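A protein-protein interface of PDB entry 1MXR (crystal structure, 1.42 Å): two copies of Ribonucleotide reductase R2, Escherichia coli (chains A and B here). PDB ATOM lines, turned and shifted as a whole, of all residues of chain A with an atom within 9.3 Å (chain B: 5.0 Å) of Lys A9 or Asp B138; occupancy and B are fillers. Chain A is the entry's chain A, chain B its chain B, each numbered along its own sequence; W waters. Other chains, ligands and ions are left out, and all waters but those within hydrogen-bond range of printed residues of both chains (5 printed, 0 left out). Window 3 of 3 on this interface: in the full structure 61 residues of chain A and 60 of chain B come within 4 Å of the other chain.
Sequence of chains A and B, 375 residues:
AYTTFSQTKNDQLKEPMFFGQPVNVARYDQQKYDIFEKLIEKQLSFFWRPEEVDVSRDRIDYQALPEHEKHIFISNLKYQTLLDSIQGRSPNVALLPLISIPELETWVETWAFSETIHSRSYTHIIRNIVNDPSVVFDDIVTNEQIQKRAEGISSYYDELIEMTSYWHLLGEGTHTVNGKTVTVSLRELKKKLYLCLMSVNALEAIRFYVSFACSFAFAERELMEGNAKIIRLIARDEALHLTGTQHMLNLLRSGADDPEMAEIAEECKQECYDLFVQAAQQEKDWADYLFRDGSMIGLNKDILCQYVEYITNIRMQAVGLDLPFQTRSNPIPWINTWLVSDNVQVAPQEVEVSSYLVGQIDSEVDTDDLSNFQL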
ATOM      1  N   PHE A   5      -6.876 -16.969   1.822  1.00  0.00           N
ATOM      2  CA  PHE A   5      -8.156 -16.407   2.207  1.00  0.00           C
ATOM      3  C   PHE A   5      -8.990 -16.113   0.962  1.00  0.00           C
ATOM      4  O   PHE A   5      -8.930 -15.018   0.396  1.00  0.00           O
ATOM      5  CB  PHE A   5      -8.040 -15.152   3.094  1.00  0.00           C
ATOM      6  CG  PHE A   5      -9.327 -14.835   3.804  1.00  0.00           C
ATOM      7  CD1 PHE A   5      -9.669 -15.439   5.034  1.00  0.00           C
ATOM      8  CD2 PHE A   5     -10.254 -13.973   3.201  1.00  0.00           C
ATOM      9  CE1 PHE A   5     -10.914 -15.184   5.634  1.00  0.00           C
ATOM     10  CE2 PHE A   5     -11.483 -13.721   3.784  1.00  0.00           C
ATOM     11  CZ  PHE A   5     -11.837 -14.305   4.995  1.00  0.00           C
ATOM     12  N   SER A   6      -9.741 -17.129   0.540  1.00  0.00           N
ATOM     13  CA  SER A   6     -10.582 -17.040  -0.663  1.00  0.00           C
ATOM     14  C   SER A   6     -11.590 -15.898  -0.467  1.00  0.00           C
ATOM     15  O   SER A   6     -12.350 -15.831   0.494  1.00  0.00           O
ATOM     16  CB  SER A   6     -11.235 -18.413  -0.899  1.00  0.00           C
ATOM     17  OG  SER A   6     -12.009 -18.838   0.228  1.00  0.00           O
ATOM     18  N   GLN A   7     -11.652 -14.995  -1.445  1.00  0.00           N
ATOM     19  CA  GLN A   7     -12.493 -13.805  -1.311  1.00  0.00           C
ATOM     20  C   GLN A   7     -13.969 -13.920  -1.698  1.00  0.00           C
ATOM     21  O   GLN A   7     -14.717 -12.951  -1.584  1.00  0.00           O
ATOM     22  CB  GLN A   7     -11.843 -12.646  -2.085  1.00  0.00           C
ATOM     23  CG  GLN A   7     -10.510 -12.175  -1.512  1.00  0.00           C
ATOM     24  CD  GLN A   7     -10.673 -11.139  -0.416  1.00  0.00           C
ATOM     25  OE1 GLN A   7     -11.613 -11.210   0.378  1.00  0.00           O
ATOM     26  NE2 GLN A   7      -9.746 -10.176  -0.355  1.00  0.00           N
ATOM     27  N   THR A   8     -14.377 -15.093  -2.145  1.00  0.00           N
ATOM     28  CA  THR A   8     -15.758 -15.353  -2.528  1.00  0.00           C
ATOM     29  C   THR A   8     -16.585 -15.791  -1.336  1.00  0.00           C
ATOM     30  O   THR A   8     -16.198 -16.720  -0.636  1.00  0.00           O
ATOM     31  CB  THR A   8     -15.823 -16.503  -3.533  1.00  0.00           C
ATOM     32  OG1 THR A   8     -15.064 -16.154  -4.695  1.00  0.00           O
ATOM     33  CG2 THR A   8     -17.261 -16.814  -3.910  1.00  0.00           C
ATOM     34  N   LYS A   9     -17.725 -15.151  -1.127  1.00  0.00           N
ATOM     35  CA  LYS A   9     -18.632 -15.513  -0.053  1.00  0.00           C
ATOM     36  C   LYS A   9     -19.324 -16.825  -0.412  1.00  0.00           C
ATOM     37  O   LYS A   9     -20.330 -16.845  -1.112  1.00  0.00           O
ATOM     38  CB  LYS A   9     -19.683 -14.407   0.165  1.00  0.00           C
ATOM     39  CG  LYS A   9     -20.528 -14.600   1.412  1.00  0.00           C
ATOM     40  CD  LYS A   9     -21.559 -13.477   1.538  1.00  0.00           C
ATOM     41  CE  LYS A   9     -22.757 -13.742   0.653  1.00  0.00           C
ATOM     42  NZ  LYS A   9     -23.518 -14.913   1.171  1.00  0.00           N
ATOM     43  N   ASN A  10     -18.805 -17.936   0.082  1.00  0.00           N
ATOM     44  CA  ASN A  10     -19.376 -19.241  -0.231  1.00  0.00           C
ATOM     45  C   ASN A  10     -20.081 -19.901   0.938  1.00  0.00           C
ATOM     46  O   ASN A  10     -19.782 -19.610   2.095  1.00  0.00           O
ATOM     47  CB  ASN A  10     -18.282 -20.161  -0.777  1.00  0.00           C
ATOM     48  CG  ASN A  10     -17.279 -20.624   0.287  1.00  0.00           C
ATOM     49  OD1 ASN A  10     -16.857 -19.850   1.165  1.00  0.00           O
ATOM     50  ND2 ASN A  10     -16.889 -21.869   0.183  1.00  0.00           N
ATOM     51  N   ASP A  11     -21.014 -20.796   0.643  1.00  0.00           N
ATOM     52  CA  ASP A  11     -21.747 -21.542   1.661  1.00  0.00           C
ATOM     53  C   ASP A  11     -20.884 -22.770   1.959  1.00  0.00           C
ATOM     54  O   ASP A  11     -20.790 -23.746   1.187  1.00  0.00           O
ATOM     55  CB  ASP A  11     -23.114 -21.998   1.117  1.00  0.00           C
ATOM     56  CG  ASP A  11     -23.956 -22.688   2.166  1.00  0.00           C
ATOM     57  OD1 ASP A  11     -23.429 -23.108   3.217  1.00  0.00           O
ATOM     58  OD2 ASP A  11     -25.177 -22.833   1.925  1.00  0.00           O
ATOM     59  N   GLN A  12     -20.243 -22.714   3.112  1.00  0.00           N
ATOM     60  CA  GLN A  12     -19.355 -23.803   3.504  1.00  0.00           C
ATOM     61  C   GLN A  12     -20.041 -25.119   3.783  1.00  0.00           C
ATOM     62  O   GLN A  12     -19.391 -26.161   3.817  1.00  0.00           O
ATOM     63  CB  GLN A  12     -18.528 -23.377   4.706  1.00  0.00           C
ATOM     64  CG  GLN A  12     -17.641 -22.173   4.460  1.00  0.00           C
ATOM     65  CD  GLN A  12     -16.937 -21.720   5.743  1.00  0.00           C
ATOM     66  OE1 GLN A  12     -17.469 -21.884   6.843  1.00  0.00           O
ATOM     67  NE2 GLN A  12     -15.759 -21.157   5.587  1.00  0.00           N
ATOM     68  N   LEU A  13     -21.361 -25.105   3.979  1.00  0.00           N
ATOM     69  CA  LEU A  13     -22.083 -26.353   4.194  1.00  0.00           C
ATOM     70  C   LEU A  13     -22.237 -27.114   2.878  1.00  0.00           C
ATOM     71  O   LEU A  13     -22.510 -28.318   2.896  1.00  0.00           O
ATOM     72  CB  LEU A  13     -23.469 -26.065   4.783  1.00  0.00           C
ATOM     73  CG  LEU A  13     -23.463 -25.329   6.122  1.00  0.00           C
ATOM     74  CD1 LEU A  13     -24.914 -25.053   6.517  1.00  0.00           C
ATOM     75  CD2 LEU A  13     -22.747 -26.152   7.210  1.00  0.00           C
ATOM     76  N   GLU A  15     -19.815 -27.148   0.282  1.00  0.00           N
ATOM     77  CA  GLU A  15     -18.575 -27.513  -0.368  1.00  0.00           C
ATOM     78  C   GLU A  15     -18.264 -28.987  -0.089  1.00  0.00           C
ATOM     79  O   GLU A  15     -18.749 -29.566   0.902  1.00  0.00           O
ATOM     80  CB  GLU A  15     -17.392 -26.733   0.262  1.00  0.00           C
ATOM     81  CG  GLU A  15     -17.423 -25.243   0.021  1.00  0.00           C
ATOM     82  CD  GLU A  15     -17.137 -24.876  -1.412  1.00  0.00           C
ATOM     83  OE1 GLU A  15     -16.373 -25.601  -2.109  1.00  0.00           O
ATOM     84  OE2 GLU A  15     -17.693 -23.810  -1.834  1.00  0.00           O
ATOM     85  N   GLN A  21     -13.652 -24.818  -2.814  1.00  0.00           N
ATOM     86  CA  GLN A  21     -13.018 -23.524  -2.543  1.00  0.00           C
ATOM     87  C   GLN A  21     -12.207 -23.593  -1.227  1.00  0.00           C
ATOM     88  O   GLN A  21     -12.707 -24.093  -0.225  1.00  0.00           O
ATOM     89  CB  GLN A  21     -14.093 -22.457  -2.413  1.00  0.00           C
ATOM     90  CG  GLN A  21     -13.536 -21.047  -2.160  1.00  0.00           C
ATOM     91  CD  GLN A  21     -14.631 -19.998  -2.057  1.00  0.00           C
ATOM     92  OE1 GLN A  21     -15.594 -20.006  -2.823  1.00  0.00           O
ATOM     93  NE2 GLN A  21     -14.507 -19.097  -1.088  1.00  0.00           N
ATOM     94  N   PRO A  22     -10.947 -23.116  -1.232  1.00  0.00           N
ATOM     95  CA  PRO A  22     -10.185 -23.164   0.029  1.00  0.00           C
ATOM     96  C   PRO A  22     -11.003 -22.429   1.096  1.00  0.00           C
ATOM     97  O   PRO A  22     -11.723 -21.446   0.815  1.00  0.00           O
ATOM     98  CB  PRO A  22      -8.898 -22.417  -0.312  1.00  0.00           C
ATOM     99  CG  PRO A  22      -8.708 -22.781  -1.769  1.00  0.00           C
ATOM    100  CD  PRO A  22     -10.104 -22.646  -2.346  1.00  0.00           C
ATOM    101  N   ASN A  24     -12.161 -19.938   3.797  1.00  0.00           N
ATOM    102  CA  ASN A  24     -11.801 -18.566   4.136  1.00  0.00           C
ATOM    103  C   ASN A  24     -12.026 -18.374   5.647  1.00  0.00           C
ATOM    104  O   ASN A  24     -11.052 -18.506   6.441  1.00  0.00           O
ATOM    105  CB  ASN A  24     -12.534 -17.496   3.236  1.00  0.00           C
ATOM    106  CG  ASN A  24     -14.018 -17.776   2.972  1.00  0.00           C
ATOM    107  OD1 ASN A  24     -14.761 -18.201   3.811  1.00  0.00           O
ATOM    108  ND2 ASN A  24     -14.456 -17.432   1.755  1.00  0.00           N
ATOM    109  N   VAL A  25     -13.249 -18.105   6.097  1.00  0.00           N
ATOM    110  CA  VAL A  25     -13.488 -17.900   7.536  1.00  0.00           C
ATOM    111  C   VAL A  25     -13.511 -19.225   8.309  1.00  0.00           C
ATOM    112  O   VAL A  25     -14.181 -20.190   7.922  1.00  0.00           O
ATOM    113  CB  VAL A  25     -14.839 -17.126   7.793  1.00  0.00           C
ATOM    114  CG1 VAL A  25     -15.993 -17.819   7.106  1.00  0.00           C
ATOM    115  CG2 VAL A  25     -15.149 -17.044   9.278  1.00  0.00           C
ATOM    116  N   ARG A  27     -14.994 -20.940  11.150  1.00  0.00           N
ATOM    117  CA  ARG A  27     -16.139 -20.809  12.048  1.00  0.00           C
ATOM    118  C   ARG A  27     -16.504 -22.201  12.530  1.00  0.00           C
ATOM    119  O   ARG A  27     -16.296 -23.181  11.799  1.00  0.00           O
ATOM    120  CB  ARG A  27     -17.326 -20.145  11.323  1.00  0.00           C
ATOM    121  CG  ARG A  27     -17.790 -20.927  10.073  1.00  0.00           C
ATOM    122  CD  ARG A  27     -18.840 -20.108   9.280  1.00  0.00           C
ATOM    123  NE  ARG A  27     -20.126 -20.039   9.972  1.00  0.00           N
ATOM    124  CZ  ARG A  27     -21.230 -19.527   9.432  1.00  0.00           C
ATOM    125  NH1 ARG A  27     -21.194 -19.031   8.197  1.00  0.00           N
ATOM    126  NH2 ARG A  27     -22.356 -19.544  10.114  1.00  0.00           N
ATOM    127  N   ASP A  29     -19.673 -22.765  14.428  1.00  0.00           N
ATOM    128  CA  ASP A  29     -21.052 -22.699  14.884  1.00  0.00           C
ATOM    129  C   ASP A  29     -21.950 -23.658  14.096  1.00  0.00           C
ATOM    130  O   ASP A  29     -23.114 -23.887  14.489  1.00  0.00           O
ATOM    131  CB  ASP A  29     -21.578 -21.279  14.691  1.00  0.00           C
ATOM    132  CG  ASP A  29     -21.527 -20.819  13.247  1.00  0.00           C
ATOM    133  OD1 ASP A  29     -20.471 -20.947  12.567  1.00  0.00           O
ATOM    134  OD2 ASP A  29     -22.555 -20.275  12.760  1.00  0.00           O
ATOM    135  N   GLN A  30     -21.416 -24.220  13.005  1.00  0.00           N
ATOM    136  CA  GLN A  30     -22.173 -25.132  12.131  1.00  0.00           C
ATOM    137  C   GLN A  30     -21.165 -26.019  11.426  1.00  0.00           C
ATOM    138  O   GLN A  30     -19.984 -25.679  11.331  1.00  0.00           O
ATOM    139  CB  GLN A  30     -22.965 -24.323  11.097  1.00  0.00           C
ATOM    140  CG  GLN A  30     -22.076 -23.437  10.256  1.00  0.00           C
ATOM    141  CD  GLN A  30     -22.781 -22.766   9.091  1.00  0.00           C
ATOM    142  OE1 GLN A  30     -22.148 -22.471   8.058  1.00  0.00           O
ATOM    143  NE2 GLN A  30     -24.069 -22.505   9.242  1.00  0.00           N
ATOM    144  N   SER B 134     -24.341 -16.451  11.528  1.00  0.00           N
ATOM    145  CA  SER B 134     -24.057 -16.373  10.107  1.00  0.00           C
ATOM    146  C   SER B 134     -23.902 -14.974   9.509  1.00  0.00           C
ATOM    147  O   SER B 134     -23.139 -14.761   8.567  1.00  0.00           O
ATOM    148  CB  SER B 134     -25.141 -17.119   9.306  1.00  0.00           C
ATOM    149  OG  SER B 134     -25.063 -18.528   9.491  1.00  0.00           O
ATOM    150  N   VAL B 135     -24.629 -14.024  10.045  1.00  0.00           N
ATOM    151  CA  VAL B 135     -24.536 -12.669   9.522  1.00  0.00           C
ATOM    152  C   VAL B 135     -23.130 -12.146   9.780  1.00  0.00           C
ATOM    153  O   VAL B 135     -22.491 -11.569   8.883  1.00  0.00           O
ATOM    154  CB  VAL B 135     -25.534 -11.730  10.209  1.00  0.00           C
ATOM    155  CG1 VAL B 135     -25.338 -10.312   9.669  1.00  0.00           C
ATOM    156  CG2 VAL B 135     -26.958 -12.197   9.974  1.00  0.00           C
ATOM    157  N   VAL B 136     -22.648 -12.373  11.003  1.00  0.00           N
ATOM    158  CA  VAL B 136     -21.326 -11.919  11.383  1.00  0.00           C
ATOM    159  C   VAL B 136     -20.269 -12.622  10.521  1.00  0.00           C
ATOM    160  O   VAL B 136     -19.410 -11.966   9.923  1.00  0.00           O
ATOM    161  CB  VAL B 136     -21.058 -12.181  12.891  1.00  0.00           C
ATOM    162  CG1 VAL B 136     -19.621 -11.785  13.246  1.00  0.00           C
ATOM    163  CG2 VAL B 136     -22.056 -11.384  13.739  1.00  0.00           C
ATOM    164  N   PHE B 137     -20.331 -13.954  10.442  1.00  0.00           N
ATOM    165  CA  PHE B 137     -19.305 -14.693   9.685  1.00  0.00           C
ATOM    166  C   PHE B 137     -19.242 -14.369   8.183  1.00  0.00           C
ATOM    167  O   PHE B 137     -18.168 -14.214   7.589  1.00  0.00           O
ATOM    168  CB  PHE B 137     -19.473 -16.205   9.903  1.00  0.00           C
ATOM    169  CG  PHE B 137     -19.088 -16.655  11.291  1.00  0.00           C
ATOM    170  CD1 PHE B 137     -17.788 -16.431  11.760  1.00  0.00           C
ATOM    171  CD2 PHE B 137     -19.991 -17.314  12.123  1.00  0.00           C
ATOM    172  CE1 PHE B 137     -17.400 -16.860  13.040  1.00  0.00           C
ATOM    173  CE2 PHE B 137     -19.615 -17.737  13.390  1.00  0.00           C
ATOM    174  CZ  PHE B 137     -18.310 -17.509  13.851  1.00  0.00           C
ATOM    175  N   ASP B 138     -20.394 -14.225   7.560  1.00  0.00           N
ATOM    176  CA  ASP B 138     -20.344 -13.885   6.143  1.00  0.00           C
ATOM    177  C   ASP B 138     -19.795 -12.469   5.921  1.00  0.00           C
ATOM    178  O   ASP B 138     -19.124 -12.219   4.920  1.00  0.00           O
ATOM    179  CB  ASP B 138     -21.736 -13.978   5.502  1.00  0.00           C
ATOM    180  CG  ASP B 138     -22.249 -15.410   5.407  1.00  0.00           C
ATOM    181  OD1 ASP B 138     -21.435 -16.341   5.173  1.00  0.00           O
ATOM    182  OD2 ASP B 138     -23.474 -15.602   5.546  1.00  0.00           O
ATOM    183  N   ASP B 139     -20.092 -11.538   6.830  1.00  0.00           N
ATOM    184  CA  ASP B 139     -19.602 -10.170   6.642  1.00  0.00           C
ATOM    185  C   ASP B 139     -18.080 -10.105   6.684  1.00  0.00           C
ATOM    186  O   ASP B 139     -17.443  -9.203   6.129  1.00  0.00           O
ATOM    187  CB  ASP B 139     -20.172  -9.210   7.692  1.00  0.00           C
ATOM    188  CG  ASP B 139     -19.895  -7.748   7.342  1.00  0.00           C
ATOM    189  OD1 ASP B 139     -20.385  -7.301   6.292  1.00  0.00           O
ATOM    190  OD2 ASP B 139     -19.167  -7.057   8.094  1.00  0.00           O
ATOM    191  N   ILE B 140     -17.471 -11.074   7.328  1.00  0.00           N
ATOM    192  CA  ILE B 140     -16.029 -11.067   7.379  1.00  0.00           C
ATOM    193  C   ILE B 140     -15.368 -11.211   6.004  1.00  0.00           C
ATOM    194  O   ILE B 140     -14.347 -10.587   5.728  1.00  0.00           O
ATOM    195  CB  ILE B 140     -15.528 -12.175   8.309  1.00  0.00           C
ATOM    196  CG1 ILE B 140     -15.913 -11.830   9.757  1.00  0.00           C
ATOM    197  CG2 ILE B 140     -14.002 -12.289   8.222  1.00  0.00           C
ATOM    198  CD1 ILE B 140     -15.723 -12.962  10.752  1.00  0.00           C
ATOM    199  N   VAL B 141     -15.945 -12.029   5.137  1.00  0.00           N
ATOM    200  CA  VAL B 141     -15.355 -12.243   3.828  1.00  0.00           C
ATOM    201  C   VAL B 141     -15.447 -11.071   2.871  1.00  0.00           C
ATOM    202  O   VAL B 141     -14.482 -10.759   2.149  1.00  0.00           O
ATOM    203  CB  VAL B 141     -16.009 -13.483   3.148  1.00  0.00           C
ATOM    204  CG1 VAL B 141     -15.507 -13.633   1.722  1.00  0.00           C
ATOM    205  CG2 VAL B 141     -15.727 -14.735   3.991  1.00  0.00           C
ATOM    206  N   THR B 142     -16.626 -10.453   2.867  1.00  0.00           N
ATOM    207  CA  THR B 142     -16.952  -9.356   1.958  1.00  0.00           C
ATOM    208  C   THR B 142     -16.887  -7.950   2.497  1.00  0.00           C
ATOM    209  O   THR B 142     -17.030  -7.007   1.717  1.00  0.00           O
ATOM    210  CB  THR B 142     -18.383  -9.506   1.415  1.00  0.00           C
ATOM    211  OG1 THR B 142     -19.308  -9.497   2.518  1.00  0.00           O
ATOM    212  CG2 THR B 142     -18.527 -10.816   0.619  1.00  0.00           C
HETATM  213  O   HOH W   1     -19.434 -18.398   5.797  1.00  0.00           O
HETATM  214  O   HOH W   2     -21.947 -18.156   3.414  1.00  0.00           O
HETATM  215  O   HOH W   3     -25.718 -21.101   7.620  1.00  0.00           O
HETATM  216  O   HOH W   4     -13.904  -8.920  -0.339  1.00  0.00           O
HETATM  217  O   HOH W   5     -23.552 -18.413   6.560  1.00  0.00           O
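Of the 9 printed residues of chain B, 5 touch a printed residue of chain A. Hydrophobic or aromatic side chains of chain B within 4 Å of the printed part of chain A: Phe B137 and Val B141. Among the printed residues, 10 pairs touch across the chains. Among the printed residues, no Asp or Glu carboxylate lies within 4 Å of a Lys or Arg side-chain nitrogen of the other chain.
No position is printed for both chains.
The backbone carbonyl oxygen of Ser A6 sits at hydrogen-bond distance from the side-chain amide nitrogen of Asn A24 (2.9 Å). O of Thr A8 lies within hydrogen-bond range of NE2 of Gln A21, at 3.0 Å. The backbone carbonyl oxygen (O) of Thr A8 lies within hydrogen-bond range of the side-chain amide nitrogen (ND2) of Asn A24, 3.0 Å away. The side-chain amide oxygen (OD1) of Asn A10 is in hydrogen-bond range of the side-chain amide nitrogen (ND2) of Asn A24. O of Val A25 lies within hydrogen-bond range of NE2 of Gln A12. NH2 of Arg A27 lies within salt-bridge range of OD2 of Asp A29 (2.8 Å).
Water W2 bridges the side-chain carboxylate of Asp B138 and the backbone carbonyl oxygen of Asn A10. Water W3 lies within hydrogen-bond range of NE2 of Gln A30 and OG of Ser B134. Water W5 lies within hydrogen-bond range of the guanidinium group (NH1) of Arg A27 (2.9 Å), the side-chain carboxylate (OD2) of Asp B138 (3.0 Å) and the side-chain hydroxyl (OG) of Ser B134 (3.3 Å). Water W1 bridges OD1 of Asp B138 and NH1 of Arg A27. Water W4 bridges the backbone carbonyl oxygen of Val B141 (3.1 Å) and the side-chain amide oxygen of Gln A7 (3.3 Å).
Printed residues of chain B within 4 Å of Gln A7: Val B141. Of the printed residues of chain B, Lys A9 touches Asp B138 (3.999 Å), Val B141 (3.9 Å) and Thr B142 (3.8 Å). Printed residues of chain A within 4 Å of Ser B134: Arg A27. Printed residues of chain A within 4 Å of Asp B138: Lys A9 (3.999 Å). Of the printed residues of chain A, Val B141 touches Gln A7, Thr A8, Lys A9 and Asn A24. The nearest printed residue of chain A that does not touch Asp B138 is Arg A27 (4.1 Å). The nearest printed residue of chain B that does not touch Arg A27 is Asp B138 (4.1 Å).
Thr A8 touches Val B141. Asp B138 touches Lys A9 (CB to CD, 3.999 Å). Val B141 touches Lys A9. CG2 of Thr B142 touches CB of Lys A9 (3.8 Å). Val B141 touches Asn A24. CG2 of Val A25 touches CD1 of Phe B137, 3.7 Å away. Phe B137 touches Arg A27. CE2 of Phe B137 touches OD1 of Asp A29, 3.4 Å away.
OE1 of Gln A7 sits close to O of Val B141 (3.4 Å). The guanidinium group (NH2) of Arg A27 is in hydrogen-bond range of the side-chain hydroxyl (OG) of Ser B134 (3.0 Å).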
